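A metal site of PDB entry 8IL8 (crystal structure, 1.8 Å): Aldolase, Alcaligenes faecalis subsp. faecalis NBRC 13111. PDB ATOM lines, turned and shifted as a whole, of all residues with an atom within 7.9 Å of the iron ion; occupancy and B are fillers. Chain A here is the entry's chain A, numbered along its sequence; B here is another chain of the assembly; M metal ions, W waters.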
ATOM      1  N   ALA A  48      -7.742   3.635   1.633  1.00  0.00           N
ATOM      2  CA  ALA A  48      -6.919   2.736   0.823  1.00  0.00           C
ATOM      3  C   ALA A  48      -6.498   1.619   1.768  1.00  0.00           C
ATOM      4  O   ALA A  48      -5.324   1.469   2.111  1.00  0.00           O
ATOM      5  CB  ALA A  48      -5.700   3.466   0.265  1.00  0.00           C
ATOM      6  N   LEU A  50      -5.902  -0.207   5.227  1.00  0.00           N
ATOM      7  CA  LEU A  50      -5.443   0.294   6.522  1.00  0.00           C
ATOM      8  C   LEU A  50      -4.177   1.186   6.376  1.00  0.00           C
ATOM      9  O   LEU A  50      -3.341   1.249   7.276  1.00  0.00           O
ATOM     10  CB  LEU A  50      -5.201  -0.903   7.469  1.00  0.00           C
ATOM     11  CG  LEU A  50      -6.450  -1.648   7.909  1.00  0.00           C
ATOM     12  CD1 LEU A  50      -6.085  -2.973   8.580  1.00  0.00           C
ATOM     13  CD2 LEU A  50      -7.347  -0.764   8.777  1.00  0.00           C
ATOM     14  N   ALA A  51      -4.045   1.885   5.246  1.00  0.00           N
ATOM     15  CA  ALA A  51      -2.885   2.720   4.998  1.00  0.00           C
ATOM     16  C   ALA A  51      -2.932   4.106   5.691  1.00  0.00           C
ATOM     17  O   ALA A  51      -1.910   4.791   5.748  1.00  0.00           O
ATOM     18  CB  ALA A  51      -2.666   2.884   3.500  1.00  0.00           C
ATOM     19  N   GLY A  52      -4.106   4.495   6.187  1.00  0.00           N
ATOM     20  CA  GLY A  52      -4.332   5.803   6.789  1.00  0.00           C
ATOM     21  C   GLY A  52      -3.731   5.918   8.170  1.00  0.00           C
ATOM     22  O   GLY A  52      -3.814   4.993   8.981  1.00  0.00           O
ATOM     23  N   GLN A  53      -3.037   7.047   8.406  1.00  0.00           N
ATOM     24  CA  GLN A  53      -2.374   7.311   9.667  1.00  0.00           C
ATOM     25  C   GLN A  53      -2.667   8.721  10.122  1.00  0.00           C
ATOM     26  O   GLN A  53      -2.746   9.653   9.316  1.00  0.00           O
ATOM     27  CB  GLN A  53      -0.874   7.181   9.491  1.00  0.00           C
ATOM     28  CG  GLN A  53      -0.401   5.866   8.890  1.00  0.00           C
ATOM     29  CD  GLN A  53       1.074   5.863   8.592  1.00  0.00           C
ATOM     30  OE1 GLN A  53       1.791   6.845   8.845  1.00  0.00           O
ATOM     31  NE2 GLN A  53       1.545   4.767   8.035  1.00  0.00           N
ATOM     32  N   ALA A 100       3.657   1.338  11.733  1.00  0.00           N
ATOM     33  CA  ALA A 100       3.966   2.159  10.567  1.00  0.00           C
ATOM     34  C   ALA A 100       4.005   3.671  10.881  1.00  0.00           C
ATOM     35  O   ALA A 100       4.520   4.435  10.084  1.00  0.00           O
ATOM     36  CB  ALA A 100       2.966   1.900   9.460  1.00  0.00           C
ATOM     37  N   PHE A 103       7.591   6.680  12.151  1.00  0.00           N
ATOM     38  CA  PHE A 103       8.326   7.725  11.439  1.00  0.00           C
ATOM     39  C   PHE A 103       7.799   9.137  11.783  1.00  0.00           C
ATOM     40  O   PHE A 103       8.548  10.098  11.656  1.00  0.00           O
ATOM     41  CB  PHE A 103       8.346   7.445   9.924  1.00  0.00           C
ATOM     42  CG  PHE A 103       7.127   7.923   9.167  1.00  0.00           C
ATOM     43  CD1 PHE A 103       7.013   9.238   8.759  1.00  0.00           C
ATOM     44  CD2 PHE A 103       6.086   7.048   8.885  1.00  0.00           C
ATOM     45  CE1 PHE A 103       5.885   9.687   8.084  1.00  0.00           C
ATOM     46  CE2 PHE A 103       4.970   7.484   8.181  1.00  0.00           C
ATOM     47  CZ  PHE A 103       4.866   8.807   7.792  1.00  0.00           C
ATOM     48  N   HIS A 119      -1.233  10.981   7.082  1.00  0.00           N
ATOM     49  CA  HIS A 119      -0.694  10.339   5.902  1.00  0.00           C
ATOM     50  C   HIS A 119      -1.786   9.384   5.360  1.00  0.00           C
ATOM     51  O   HIS A 119      -2.264   8.504   6.077  1.00  0.00           O
ATOM     52  CB  HIS A 119       0.622   9.570   6.210  1.00  0.00           C
ATOM     53  CG  HIS A 119       0.980   8.606   5.119  1.00  0.00           C
ATOM     54  ND1 HIS A 119       1.234   9.040   3.821  1.00  0.00           N
ATOM     55  CD2 HIS A 119       1.062   7.250   5.147  1.00  0.00           C
ATOM     56  CE1 HIS A 119       1.475   7.933   3.118  1.00  0.00           C
ATOM     57  NE2 HIS A 119       1.385   6.852   3.874  1.00  0.00           N
ATOM     58  N   THR A 120      -2.142   9.510   4.101  1.00  0.00           N
ATOM     59  CA  THR A 120      -3.075   8.577   3.462  1.00  0.00           C
ATOM     60  C   THR A 120      -2.617   8.371   1.993  1.00  0.00           C
ATOM     61  O   THR A 120      -1.719   9.079   1.508  1.00  0.00           O
ATOM     62  CB  THR A 120      -4.603   9.054   3.544  1.00  0.00           C
ATOM     63  OG1 THR A 120      -4.858   9.994   2.527  1.00  0.00           O
ATOM     64  CG2 THR A 120      -4.993   9.714   4.858  1.00  0.00           C
ATOM     65  N   HIS A 121      -3.253   7.415   1.296  1.00  0.00           N
ATOM     66  CA  HIS A 121      -3.033   7.209  -0.122  1.00  0.00           C
ATOM     67  C   HIS A 121      -4.398   7.559  -0.753  1.00  0.00           C
ATOM     68  O   HIS A 121      -5.021   6.724  -1.384  1.00  0.00           O
ATOM     69  CB  HIS A 121      -2.664   5.747  -0.444  1.00  0.00           C
ATOM     70  CG  HIS A 121      -1.511   5.164   0.324  1.00  0.00           C
ATOM     71  ND1 HIS A 121      -1.275   3.794   0.294  1.00  0.00           N
ATOM     72  CD2 HIS A 121      -0.543   5.751   1.064  1.00  0.00           C
ATOM     73  CE1 HIS A 121      -0.216   3.594   1.044  1.00  0.00           C
ATOM     74  NE2 HIS A 121       0.273   4.738   1.525  1.00  0.00           N
ATOM     75  N   TRP A 155      10.951   6.879  -4.515  1.00  0.00           N
ATOM     76  CA  TRP A 155      10.132   5.962  -3.761  1.00  0.00           C
ATOM     77  C   TRP A 155      11.072   4.964  -3.075  1.00  0.00           C
ATOM     78  O   TRP A 155      11.755   4.186  -3.743  1.00  0.00           O
ATOM     79  CB  TRP A 155       9.143   5.205  -4.679  1.00  0.00           C
ATOM     80  CG  TRP A 155       8.272   4.240  -3.936  1.00  0.00           C
ATOM     81  CD1 TRP A 155       7.488   4.514  -2.850  1.00  0.00           C
ATOM     82  CD2 TRP A 155       8.110   2.838  -4.205  1.00  0.00           C
ATOM     83  NE1 TRP A 155       6.863   3.362  -2.415  1.00  0.00           N
ATOM     84  CE2 TRP A 155       7.219   2.330  -3.247  1.00  0.00           C
ATOM     85  CE3 TRP A 155       8.630   1.971  -5.171  1.00  0.00           C
ATOM     86  CZ2 TRP A 155       6.808   0.989  -3.239  1.00  0.00           C
ATOM     87  CZ3 TRP A 155       8.266   0.633  -5.142  1.00  0.00           C
ATOM     88  CH2 TRP A 155       7.353   0.160  -4.191  1.00  0.00           C
ATOM     89  N   GLY A 157      10.225   2.321  -1.283  1.00  0.00           N
ATOM     90  CA  GLY A 157       9.637   0.991  -1.126  1.00  0.00           C
ATOM     91  C   GLY A 157       9.043   0.760   0.248  1.00  0.00           C
ATOM     92  O   GLY A 157       8.383   1.633   0.786  1.00  0.00           O
ATOM     93  N   PRO A 159       9.670   0.723   3.864  1.00  0.00           N
ATOM     94  CA  PRO A 159      10.741   1.412   4.596  1.00  0.00           C
ATOM     95  C   PRO A 159      10.936   0.951   6.016  1.00  0.00           C
ATOM     96  O   PRO A 159      10.052   0.356   6.614  1.00  0.00           O
ATOM     97  CB  PRO A 159      10.252   2.838   4.596  1.00  0.00           C
ATOM     98  CG  PRO A 159       8.724   2.691   4.643  1.00  0.00           C
ATOM     99  CD  PRO A 159       8.350   1.322   4.155  1.00  0.00           C
ATOM    100  N   GLU A 164      12.541   5.931   6.647  1.00  0.00           N
ATOM    101  CA  GLU A 164      11.350   6.670   6.239  1.00  0.00           C
ATOM    102  C   GLU A 164      11.258   8.067   6.876  1.00  0.00           C
ATOM    103  O   GLU A 164      11.087   9.033   6.163  1.00  0.00           O
ATOM    104  CB  GLU A 164      10.061   5.874   6.466  1.00  0.00           C
ATOM    105  CG  GLU A 164       8.848   6.591   5.899  1.00  0.00           C
ATOM    106  CD  GLU A 164       7.616   5.733   5.782  1.00  0.00           C
ATOM    107  OE1 GLU A 164       7.397   4.880   6.671  1.00  0.00           O
ATOM    108  OE2 GLU A 164       6.855   5.919   4.800  1.00  0.00           O
ATOM    109  N   ILE A 168      11.451  11.438   4.752  1.00  0.00           N
ATOM    110  CA  ILE A 168      10.296  12.338   4.708  1.00  0.00           C
ATOM    111  C   ILE A 168      10.554  13.659   5.418  1.00  0.00           C
ATOM    112  O   ILE A 168      10.199  14.685   4.841  1.00  0.00           O
ATOM    113  CB  ILE A 168       8.993  11.630   5.179  1.00  0.00           C
ATOM    114  CG1 ILE A 168       8.569  10.576   4.143  1.00  0.00           C
ATOM    115  CG2 ILE A 168       7.847  12.628   5.427  1.00  0.00           C
ATOM    116  CD1 ILE A 168       7.434   9.720   4.567  1.00  0.00           C
ATOM    117  N   LEU A 180       4.283  12.205  -2.084  1.00  0.00           N
ATOM    118  CA  LEU A 180       5.293  11.135  -1.990  1.00  0.00           C
ATOM    119  C   LEU A 180       5.160  10.271  -3.221  1.00  0.00           C
ATOM    120  O   LEU A 180       4.196   9.521  -3.309  1.00  0.00           O
ATOM    121  CB  LEU A 180       4.996  10.286  -0.743  1.00  0.00           C
ATOM    122  CG  LEU A 180       4.935  11.067   0.587  1.00  0.00           C
ATOM    123  CD1 LEU A 180       4.324  10.228   1.695  1.00  0.00           C
ATOM    124  CD2 LEU A 180       6.325  11.538   1.004  1.00  0.00           C
ATOM    125  N   HIS A 183       3.275   6.709  -3.993  1.00  0.00           N
ATOM    126  CA  HIS A 183       2.859   6.352  -2.647  1.00  0.00           C
ATOM    127  C   HIS A 183       1.571   7.058  -2.201  1.00  0.00           C
ATOM    128  O   HIS A 183       0.532   6.407  -2.131  1.00  0.00           O
ATOM    129  CB  HIS A 183       4.057   6.609  -1.699  1.00  0.00           C
ATOM    130  CG  HIS A 183       3.840   6.240  -0.263  1.00  0.00           C
ATOM    131  ND1 HIS A 183       4.770   6.544   0.689  1.00  0.00           N
ATOM    132  CD2 HIS A 183       2.807   5.576   0.317  1.00  0.00           C
ATOM    133  CE1 HIS A 183       4.283   6.091   1.831  1.00  0.00           C
ATOM    134  NE2 HIS A 183       3.100   5.529   1.660  1.00  0.00           N
ATOM    135  N   GLY A 184       1.629   8.345  -1.890  1.00  0.00           N
ATOM    136  CA  GLY A 184       0.491   9.121  -1.442  1.00  0.00           C
ATOM    137  C   GLY A 184       0.926  10.510  -1.030  1.00  0.00           C
ATOM    138  O   GLY A 184       1.708  11.154  -1.746  1.00  0.00           O
ATOM    139  N   TYR A 185       0.429  11.000   0.099  1.00  0.00           N
ATOM    140  CA  TYR A 185       0.805  12.334   0.558  1.00  0.00           C
ATOM    141  C   TYR A 185       0.933  12.349   2.091  1.00  0.00           C
ATOM    142  O   TYR A 185       0.474  11.421   2.774  1.00  0.00           O
ATOM    143  CB  TYR A 185      -0.235  13.399   0.062  1.00  0.00           C
ATOM    144  CG  TYR A 185      -1.479  13.408   0.928  1.00  0.00           C
ATOM    145  CD1 TYR A 185      -1.523  14.122   2.119  1.00  0.00           C
ATOM    146  CD2 TYR A 185      -2.594  12.634   0.584  1.00  0.00           C
ATOM    147  CE1 TYR A 185      -2.571  13.985   2.997  1.00  0.00           C
ATOM    148  CE2 TYR A 185      -3.691  12.571   1.437  1.00  0.00           C
ATOM    149  CZ  TYR A 185      -3.682  13.268   2.643  1.00  0.00           C
ATOM    150  OH  TYR A 185      -4.722  13.217   3.535  1.00  0.00           O
ATOM    151  N   GLN B 139       2.612   2.305  -8.138  1.00  0.00           N
ATOM    152  CA  GLN B 139       2.256   2.870  -6.840  1.00  0.00           C
ATOM    153  C   GLN B 139       2.167   1.764  -5.802  1.00  0.00           C
ATOM    154  O   GLN B 139       1.903   0.602  -6.144  1.00  0.00           O
ATOM    155  CB  GLN B 139       0.927   3.671  -6.963  1.00  0.00           C
ATOM    156  CG  GLN B 139       0.539   4.496  -5.715  1.00  0.00           C
ATOM    157  CD  GLN B 139      -0.384   3.731  -4.787  1.00  0.00           C
ATOM    158  OE1 GLN B 139      -0.981   2.704  -5.165  1.00  0.00           O
ATOM    159  NE2 GLN B 139      -0.484   4.134  -3.548  1.00  0.00           N
ATOM    160  N   MET B 140       2.494   2.097  -4.537  1.00  0.00           N
ATOM    161  CA  MET B 140       2.502   1.198  -3.382  1.00  0.00           C
ATOM    162  C   MET B 140       1.339   0.159  -3.346  1.00  0.00           C
ATOM    163  O   MET B 140       1.604  -1.019  -3.179  1.00  0.00           O
ATOM    164  CB  MET B 140       2.528   2.044  -2.085  1.00  0.00           C
ATOM    165  CG  MET B 140       2.509   1.219  -0.845  1.00  0.00           C
ATOM    166  SD  MET B 140       3.974   0.152  -0.641  1.00  0.00           S
ATOM    167  CE  MET B 140       3.503  -0.687   0.831  1.00  0.00           C
ATOM    168  N   ASP B 141       0.089   0.612  -3.469  1.00  0.00           N
ATOM    169  CA  ASP B 141      -1.104  -0.237  -3.415  1.00  0.00           C
ATOM    170  C   ASP B 141      -1.347  -1.089  -4.671  1.00  0.00           C
ATOM    171  O   ASP B 141      -2.247  -1.905  -4.674  1.00  0.00           O
ATOM    172  CB  ASP B 141      -2.357   0.594  -3.085  1.00  0.00           C
ATOM    173  CG  ASP B 141      -2.154   1.349  -1.788  1.00  0.00           C
ATOM    174  OD1 ASP B 141      -1.569   0.765  -0.855  1.00  0.00           O
ATOM    175  OD2 ASP B 141      -2.542   2.550  -1.732  1.00  0.00           O
HETATM  176 FE    FE M   1       1.716   4.759   3.218  1.00  0.00          FE
HETATM  177  O   HOH W   1       2.230   2.731   2.619  1.00  0.00           O
HETATM  178  O   HOH W   2       0.300   3.955   5.006  1.00  0.00           O
HETATM  179  O   HOH W   3       3.388   4.832   4.553  1.00  0.00           O
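The iron ion is bound by water W3 (2.1 Å). The iron ion is bound by water W1, at 2.2 Å. NE2 of His 119 binds the iron ion (2.2 Å). NE2 of His 183 is bound to the iron ion (2.2 Å). NE2 of His 121 binds the iron ion, at 2.2 Å. Water W2 is bound to the iron ion. The iron ion has six donor atoms within binding distance.
The backbone NH of Gln 53 sits at hydrogen-bond distance from the backbone carbonyl oxygen of His 119. The backbone carbonyl oxygen (O) of Tyr 185 lies within hydrogen-bond range of a ring nitrogen (ND1) of His 119 (2.7 Å). The backbone carbonyl oxygen of His 183 is in hydrogen-bond range of the side-chain amide nitrogen of Gln 139 of chain B (2.9 Å). OD2 of Asp 141 of chain B is in hydrogen-bond range of ND1 of His 121 (2.7 Å).
Water W2 bridges O of Ala 51 (2.5 Å) and NE2 of Gln 53 (3.4 Å).
Three residues have an atom within 4 Å of the iron ion: His 119, His 121 and His 183. The nearest printed residue that does not touch the iron ion is Ala 51 (4.4 Å).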
